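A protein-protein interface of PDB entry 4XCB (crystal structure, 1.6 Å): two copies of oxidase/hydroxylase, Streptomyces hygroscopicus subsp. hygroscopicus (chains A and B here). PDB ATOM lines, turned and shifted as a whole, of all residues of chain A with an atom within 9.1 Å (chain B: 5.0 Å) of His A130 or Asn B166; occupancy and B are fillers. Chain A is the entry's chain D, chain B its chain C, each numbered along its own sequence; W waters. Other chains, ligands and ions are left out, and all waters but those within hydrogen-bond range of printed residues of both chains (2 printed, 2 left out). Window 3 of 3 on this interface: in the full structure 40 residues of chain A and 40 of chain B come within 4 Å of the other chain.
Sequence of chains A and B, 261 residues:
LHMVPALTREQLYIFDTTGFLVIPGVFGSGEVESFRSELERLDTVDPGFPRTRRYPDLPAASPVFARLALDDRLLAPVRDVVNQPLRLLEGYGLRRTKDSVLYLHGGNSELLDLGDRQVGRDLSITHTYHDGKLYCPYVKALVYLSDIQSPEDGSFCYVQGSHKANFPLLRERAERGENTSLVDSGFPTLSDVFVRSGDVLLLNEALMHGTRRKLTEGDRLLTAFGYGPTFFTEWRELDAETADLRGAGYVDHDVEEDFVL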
ATOM      1  N   ASP A  16      22.990 -14.126 -29.309  1.00  0.00           N
ATOM      2  CA  ASP A  16      22.731 -14.900 -28.106  1.00  0.00           C
ATOM      3  C   ASP A  16      24.021 -15.248 -27.386  1.00  0.00           C
ATOM      4  O   ASP A  16      24.140 -15.040 -26.184  1.00  0.00           O
ATOM      5  CB  ASP A  16      21.970 -16.173 -28.448  1.00  0.00           C
ATOM      6  CG  ASP A  16      21.853 -17.121 -27.275  1.00  0.00           C
ATOM      7  OD1 ASP A  16      21.386 -16.707 -26.193  1.00  0.00           O
ATOM      8  OD2 ASP A  16      22.243 -18.294 -27.437  1.00  0.00           O
ATOM      9  N   ASN A  83      11.504  -9.086 -28.700  1.00  0.00           N
ATOM     10  CA  ASN A  83      10.275  -9.861 -28.856  1.00  0.00           C
ATOM     11  C   ASN A  83       9.208  -9.487 -27.827  1.00  0.00           C
ATOM     12  O   ASN A  83       8.565 -10.345 -27.205  1.00  0.00           O
ATOM     13  CB  ASN A  83      10.604 -11.356 -28.816  1.00  0.00           C
ATOM     14  CG  ASN A  83      11.212 -11.831 -30.114  1.00  0.00           C
ATOM     15  OD1 ASN A  83      10.560 -11.799 -31.148  1.00  0.00           O
ATOM     16  ND2 ASN A  83      12.478 -12.279 -30.072  1.00  0.00           N
ATOM     17  N   GLN A  84       9.054  -8.180 -27.642  1.00  0.00           N
ATOM     18  CA  GLN A  84       8.009  -7.612 -26.808  1.00  0.00           C
ATOM     19  C   GLN A  84       7.414  -6.425 -27.552  1.00  0.00           C
ATOM     20  O   GLN A  84       8.056  -5.860 -28.439  1.00  0.00           O
ATOM     21  CB  GLN A  84       8.555  -7.163 -25.449  1.00  0.00           C
ATOM     22  CG  GLN A  84       9.163  -8.280 -24.604  1.00  0.00           C
ATOM     23  CD  GLN A  84       8.110  -9.124 -23.927  1.00  0.00           C
ATOM     24  OE1 GLN A  84       7.587  -8.770 -22.867  1.00  0.00           O
ATOM     25  NE2 GLN A  84       7.777 -10.246 -24.546  1.00  0.00           N
ATOM     26  N   HIS A 127      17.702 -11.027 -18.993  1.00  0.00           N
ATOM     27  CA  HIS A 127      17.140 -11.511 -20.245  1.00  0.00           C
ATOM     28  C   HIS A 127      16.979 -13.020 -20.239  1.00  0.00           C
ATOM     29  O   HIS A 127      17.556 -13.711 -19.406  1.00  0.00           O
ATOM     30  CB  HIS A 127      18.022 -11.080 -21.416  1.00  0.00           C
ATOM     31  CG  HIS A 127      19.446 -11.511 -21.277  1.00  0.00           C
ATOM     32  ND1 HIS A 127      19.936 -12.649 -21.876  1.00  0.00           N
ATOM     33  CD2 HIS A 127      20.476 -10.971 -20.585  1.00  0.00           C
ATOM     34  CE1 HIS A 127      21.219 -12.785 -21.578  1.00  0.00           C
ATOM     35  NE2 HIS A 127      21.569 -11.785 -20.789  1.00  0.00           N
ATOM     36  N   THR A 128      16.158 -13.526 -21.150  1.00  0.00           N
ATOM     37  CA  THR A 128      15.915 -14.958 -21.171  1.00  0.00           C
ATOM     38  C   THR A 128      15.670 -15.438 -22.593  1.00  0.00           C
ATOM     39  O   THR A 128      15.876 -14.700 -23.556  1.00  0.00           O
ATOM     40  CB  THR A 128      14.728 -15.332 -20.242  1.00  0.00           C
ATOM     41  OG1 THR A 128      14.571 -16.752 -20.190  1.00  0.00           O
ATOM     42  CG2 THR A 128      13.432 -14.676 -20.723  1.00  0.00           C
ATOM     43  N   TYR A 129      15.270 -16.701 -22.711  1.00  0.00           N
ATOM     44  CA  TYR A 129      15.070 -17.356 -23.984  1.00  0.00           C
ATOM     45  C   TYR A 129      13.939 -18.339 -23.796  1.00  0.00           C
ATOM     46  O   TYR A 129      13.880 -19.027 -22.767  1.00  0.00           O
ATOM     47  CB  TYR A 129      16.335 -18.093 -24.448  1.00  0.00           C
ATOM     48  CG  TYR A 129      16.096 -19.026 -25.608  1.00  0.00           C
ATOM     49  CD1 TYR A 129      15.694 -20.343 -25.401  1.00  0.00           C
ATOM     50  CD2 TYR A 129      16.247 -18.587 -26.911  1.00  0.00           C
ATOM     51  CE1 TYR A 129      15.464 -21.193 -26.460  1.00  0.00           C
ATOM     52  CE2 TYR A 129      16.012 -19.426 -27.966  1.00  0.00           C
ATOM     53  CZ  TYR A 129      15.618 -20.730 -27.732  1.00  0.00           C
ATOM     54  OH  TYR A 129      15.405 -21.565 -28.795  1.00  0.00           O
ATOM     55  N   HIS A 130      13.056 -18.425 -24.785  1.00  0.00           N
ATOM     56  CA  HIS A 130      11.928 -19.324 -24.679  1.00  0.00           C
ATOM     57  C   HIS A 130      11.373 -19.645 -26.042  1.00  0.00           C
ATOM     58  O   HIS A 130      11.018 -18.736 -26.801  1.00  0.00           O
ATOM     59  CB  HIS A 130      10.849 -18.707 -23.792  1.00  0.00           C
ATOM     60  CG  HIS A 130       9.638 -19.568 -23.614  1.00  0.00           C
ATOM     61  ND1 HIS A 130       9.645 -20.726 -22.867  1.00  0.00           N
ATOM     62  CD2 HIS A 130       8.363 -19.409 -24.052  1.00  0.00           C
ATOM     63  CE1 HIS A 130       8.435 -21.263 -22.880  1.00  0.00           C
ATOM     64  NE2 HIS A 130       7.636 -20.476 -23.581  1.00  0.00           N
ATOM     65  N   ASP A 131      11.320 -20.942 -26.341  1.00  0.00           N
ATOM     66  CA  ASP A 131      10.659 -21.462 -27.535  1.00  0.00           C
ATOM     67  C   ASP A 131      11.124 -20.751 -28.801  1.00  0.00           C
ATOM     68  O   ASP A 131      10.310 -20.228 -29.568  1.00  0.00           O
ATOM     69  CB  ASP A 131       9.127 -21.348 -27.386  1.00  0.00           C
ATOM     70  CG  ASP A 131       8.558 -22.378 -26.424  1.00  0.00           C
ATOM     71  OD1 ASP A 131       9.352 -23.144 -25.835  1.00  0.00           O
ATOM     72  OD2 ASP A 131       7.314 -22.425 -26.261  1.00  0.00           O
ATOM     73  N   GLY A 132      12.436 -20.707 -29.003  1.00  0.00           N
ATOM     74  CA  GLY A 132      12.995 -20.228 -30.252  1.00  0.00           C
ATOM     75  C   GLY A 132      13.176 -18.727 -30.326  1.00  0.00           C
ATOM     76  O   GLY A 132      13.555 -18.214 -31.371  1.00  0.00           O
ATOM     77  N   LYS A 133      12.917 -18.029 -29.223  1.00  0.00           N
ATOM     78  CA  LYS A 133      13.019 -16.576 -29.204  1.00  0.00           C
ATOM     79  C   LYS A 133      13.821 -16.022 -28.025  1.00  0.00           C
ATOM     80  O   LYS A 133      13.697 -16.496 -26.889  1.00  0.00           O
ATOM     81  CB  LYS A 133      11.612 -15.960 -29.186  1.00  0.00           C
ATOM     82  CG  LYS A 133      10.800 -16.227 -30.432  1.00  0.00           C
ATOM     83  CD  LYS A 133       9.544 -15.373 -30.408  1.00  0.00           C
ATOM     84  CE  LYS A 133       8.791 -15.478 -31.715  1.00  0.00           C
ATOM     85  NZ  LYS A 133       8.283 -16.854 -31.915  1.00  0.00           N
ATOM     86  N   LEU A 134      14.632 -15.003 -28.309  1.00  0.00           N
ATOM     87  CA  LEU A 134      15.303 -14.216 -27.287  1.00  0.00           C
ATOM     88  C   LEU A 134      14.379 -13.165 -26.697  1.00  0.00           C
ATOM     89  O   LEU A 134      13.567 -12.565 -27.407  1.00  0.00           O
ATOM     90  CB  LEU A 134      16.546 -13.544 -27.876  1.00  0.00           C
ATOM     91  CG  LEU A 134      17.621 -14.508 -28.350  1.00  0.00           C
ATOM     92  CD1 LEU A 134      18.671 -13.775 -29.195  1.00  0.00           C
ATOM     93  CD2 LEU A 134      18.269 -15.152 -27.149  1.00  0.00           C
ATOM     94  N   TYR A 135      14.505 -12.944 -25.394  1.00  0.00           N
ATOM     95  CA  TYR A 135      13.745 -11.904 -24.711  1.00  0.00           C
ATOM     96  C   TYR A 135      14.705 -11.036 -23.905  1.00  0.00           C
ATOM     97  O   TYR A 135      14.965 -11.289 -22.735  1.00  0.00           O
ATOM     98  CB  TYR A 135      12.650 -12.518 -23.827  1.00  0.00           C
ATOM     99  CG  TYR A 135      11.580 -13.240 -24.625  1.00  0.00           C
ATOM    100  CD1 TYR A 135      10.509 -12.546 -25.189  1.00  0.00           C
ATOM    101  CD2 TYR A 135      11.636 -14.614 -24.817  1.00  0.00           C
ATOM    102  CE1 TYR A 135       9.529 -13.207 -25.926  1.00  0.00           C
ATOM    103  CE2 TYR A 135      10.663 -15.285 -25.547  1.00  0.00           C
ATOM    104  CZ  TYR A 135       9.603 -14.568 -26.092  1.00  0.00           C
ATOM    105  OH  TYR A 135       8.645 -15.231 -26.814  1.00  0.00           O
ATOM    106  N   CYS A 136      15.252 -10.016 -24.557  1.00  0.00           N
ATOM    107  CA  CYS A 136      16.135  -9.073 -23.898  1.00  0.00           C
ATOM    108  C   CYS A 136      15.374  -7.768 -23.672  1.00  0.00           C
ATOM    109  O   CYS A 136      14.893  -7.178 -24.627  1.00  0.00           O
ATOM    110  CB  CYS A 136      17.384  -8.830 -24.736  1.00  0.00           C
ATOM    111  SG  CYS A 136      18.238 -10.369 -25.233  1.00  0.00           S
ATOM    112  N   SER B 109       3.612 -18.505 -19.173  1.00  0.00           N
ATOM    113  CA  SER B 109       3.921 -18.858 -20.547  1.00  0.00           C
ATOM    114  C   SER B 109       2.740 -18.725 -21.489  1.00  0.00           C
ATOM    115  O   SER B 109       2.723 -19.352 -22.546  1.00  0.00           O
ATOM    116  CB  SER B 109       4.454 -20.294 -20.626  1.00  0.00           C
ATOM    117  OG  SER B 109       5.795 -20.371 -20.175  1.00  0.00           O
ATOM    118  N   GLY B 120       5.737 -15.911 -26.134  1.00  0.00           N
ATOM    119  CA  GLY B 120       5.276 -16.687 -24.992  1.00  0.00           C
ATOM    120  C   GLY B 120       5.941 -16.329 -23.671  1.00  0.00           C
ATOM    121  O   GLY B 120       5.906 -17.093 -22.709  1.00  0.00           O
ATOM    122  N   ARG B 121       6.575 -15.164 -23.632  1.00  0.00           N
ATOM    123  CA  ARG B 121       7.079 -14.593 -22.392  1.00  0.00           C
ATOM    124  C   ARG B 121       6.561 -13.162 -22.258  1.00  0.00           C
ATOM    125  O   ARG B 121       6.523 -12.433 -23.243  1.00  0.00           O
ATOM    126  CB  ARG B 121       8.611 -14.598 -22.367  1.00  0.00           C
ATOM    127  CG  ARG B 121       9.221 -15.932 -21.964  1.00  0.00           C
ATOM    128  CD  ARG B 121       9.060 -16.143 -20.464  1.00  0.00           C
ATOM    129  NE  ARG B 121       9.563 -17.444 -20.032  1.00  0.00           N
ATOM    130  CZ  ARG B 121       8.877 -18.576 -20.153  1.00  0.00           C
ATOM    131  NH1 ARG B 121       7.673 -18.554 -20.703  1.00  0.00           N
ATOM    132  NH2 ARG B 121       9.386 -19.726 -19.730  1.00  0.00           N
ATOM    133  N   LYS B 164       5.440 -20.745 -12.786  1.00  0.00           N
ATOM    134  CA  LYS B 164       6.691 -21.259 -13.380  1.00  0.00           C
ATOM    135  C   LYS B 164       6.403 -22.186 -14.563  1.00  0.00           C
ATOM    136  O   LYS B 164       7.262 -22.998 -14.977  1.00  0.00           O
ATOM    137  CB  LYS B 164       7.549 -21.990 -12.334  1.00  0.00           C
ATOM    138  CG  LYS B 164       8.034 -21.067 -11.188  1.00  0.00           C
ATOM    139  CD  LYS B 164       8.789 -21.848 -10.121  1.00  0.00           C
ATOM    140  CE  LYS B 164       9.457 -20.943  -9.085  1.00  0.00           C
ATOM    141  NZ  LYS B 164      10.032 -21.755  -7.974  1.00  0.00           N
ATOM    142  N   ALA B 165       5.197 -22.078 -15.108  1.00  0.00           N
ATOM    143  CA  ALA B 165       4.781 -22.872 -16.265  1.00  0.00           C
ATOM    144  C   ALA B 165       5.647 -22.596 -17.489  1.00  0.00           C
ATOM    145  O   ALA B 165       5.999 -21.444 -17.772  1.00  0.00           O
ATOM    146  CB  ALA B 165       3.313 -22.601 -16.606  1.00  0.00           C
ATOM    147  N   ASN B 166       5.965 -23.659 -18.217  1.00  0.00           N
ATOM    148  CA  ASN B 166       6.699 -23.556 -19.469  1.00  0.00           C
ATOM    149  C   ASN B 166       5.801 -23.696 -20.701  1.00  0.00           C
ATOM    150  O   ASN B 166       6.219 -23.387 -21.812  1.00  0.00           O
ATOM    151  CB  ASN B 166       7.810 -24.614 -19.497  1.00  0.00           C
ATOM    152  CG  ASN B 166       8.938 -24.278 -18.560  1.00  0.00           C
ATOM    153  OD1 ASN B 166       9.536 -23.210 -18.668  1.00  0.00           O
ATOM    154  ND2 ASN B 166       9.230 -25.170 -17.623  1.00  0.00           N
ATOM    155  N   PHE B 167       4.553 -24.138 -20.494  1.00  0.00           N
ATOM    156  CA  PHE B 167       3.609 -24.370 -21.583  1.00  0.00           C
ATOM    157  C   PHE B 167       2.424 -23.414 -21.423  1.00  0.00           C
ATOM    158  O   PHE B 167       2.072 -23.077 -20.296  1.00  0.00           O
ATOM    159  CB  PHE B 167       3.079 -25.812 -21.584  1.00  0.00           C
ATOM    160  CG  PHE B 167       4.123 -26.865 -21.829  1.00  0.00           C
ATOM    161  CD1 PHE B 167       4.585 -27.113 -23.111  1.00  0.00           C
ATOM    162  CD2 PHE B 167       4.604 -27.638 -20.787  1.00  0.00           C
ATOM    163  CE1 PHE B 167       5.532 -28.100 -23.345  1.00  0.00           C
ATOM    164  CE2 PHE B 167       5.557 -28.633 -21.017  1.00  0.00           C
ATOM    165  CZ  PHE B 167       6.016 -28.858 -22.291  1.00  0.00           C
ATOM    166  N   PRO B 168       1.817 -22.993 -22.544  1.00  0.00           N
ATOM    167  CA  PRO B 168       0.595 -22.177 -22.474  1.00  0.00           C
ATOM    168  C   PRO B 168      -0.640 -23.052 -22.255  1.00  0.00           C
ATOM    169  O   PRO B 168      -0.710 -24.168 -22.786  1.00  0.00           O
ATOM    170  CB  PRO B 168       0.558 -21.486 -23.842  1.00  0.00           C
ATOM    171  CG  PRO B 168       1.239 -22.443 -24.751  1.00  0.00           C
ATOM    172  CD  PRO B 168       2.322 -23.111 -23.923  1.00  0.00           C
HETATM  173  O   HOH W   1       5.671 -23.306 -24.494  1.00  0.00           O
HETATM  174  O   HOH W   2       4.780 -20.218 -24.241  1.00  0.00           O
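Of the 8 printed residues of chain B, 4 touch a printed residue of chain A. Of the 13 printed residues of chain A, 3 touch a printed residue of chain B. Hydrophobic or aromatic side chains of chain A that line the printed part of chain B: His A130 and Tyr A135. Among the printed residues, no Asp or Glu carboxylate lies within 4 Å of a Lys or Arg side-chain nitrogen of the other chain.
Of the printed residues of chain B, Gln A84 touches Arg B121. His A130 touches just these residues of chain B: Ser B109, Gly B120, Arg B121 and Asn B166. Of the printed residues of chain B, Tyr A135 touches Gly B120 and Arg B121. Printed residues of chain A within 4 Å of Ser B109: His A130. Gly B120 touches just these residues of chain A: His A130 and Tyr A135. Printed residues of chain A within 4 Å of Arg B121: Gln A84 (2.8 Å), His A130 (3.3 Å) and Tyr A135 (3.8 Å). Of chain A, only His A130 (3.3 Å) comes within 4 Å of Asn B166. The nearest residue of chain A that does not touch Asn B166 is Asp A131 (4.7 Å). The nearest printed residue of chain B that does not touch Tyr A135 is Ser B109 (8.4 Å).
OH of Tyr A135 sits at hydrogen-bond distance from N of Gly B120 (3.1 Å). The side-chain amide nitrogen (NE2) of Gln A84 sits at hydrogen-bond distance from the backbone carbonyl oxygen (O) of Arg B121 (2.8 Å). A ring nitrogen (ND1) of His A130 lies within hydrogen-bond range of the guanidinium group (NH2) of Arg B121, at 3.3 Å.
OG of Ser B109 is in hydrogen-bond range of NH1 of Arg B121 (2.7 Å). OG of Ser B109 is in hydrogen-bond range of O of Ala B165 (2.6 Å). The side-chain hydroxyl of Ser B109 lies close to the backbone carbonyl oxygen of Asn B166 (3.5 Å). The backbone NH of Tyr A135 is in hydrogen-bond range of the backbone carbonyl oxygen of Thr A128, at 2.9 Å. A ring nitrogen (NE2) of His A130 lies within hydrogen-bond range of the side-chain carboxylate (OD2) of Asp A131 (3.3 Å).
No position is printed for both chains. Of the 7 pairs that touch across the chains among the printed residues, none has its exchanged pair printed and touching as well.
Ser B109 touches His A130 (OG to NE2, 3.9 Å). His A130 touches Gly B120 (CD2 to O, 3.6 Å). Asn B166 touches His A130 (O to CE1, 3.3 Å). Arg B121 touches Tyr A135 (N to OH, 3.8 Å).
Water W1 lies within hydrogen-bond range of the side-chain carboxylate of Asp A131 and the backbone carbonyl oxygen of Asn B166. Water W2 bridges the backbone carbonyl oxygen of Ser B109 and a ring nitrogen (NE2) of His A130.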
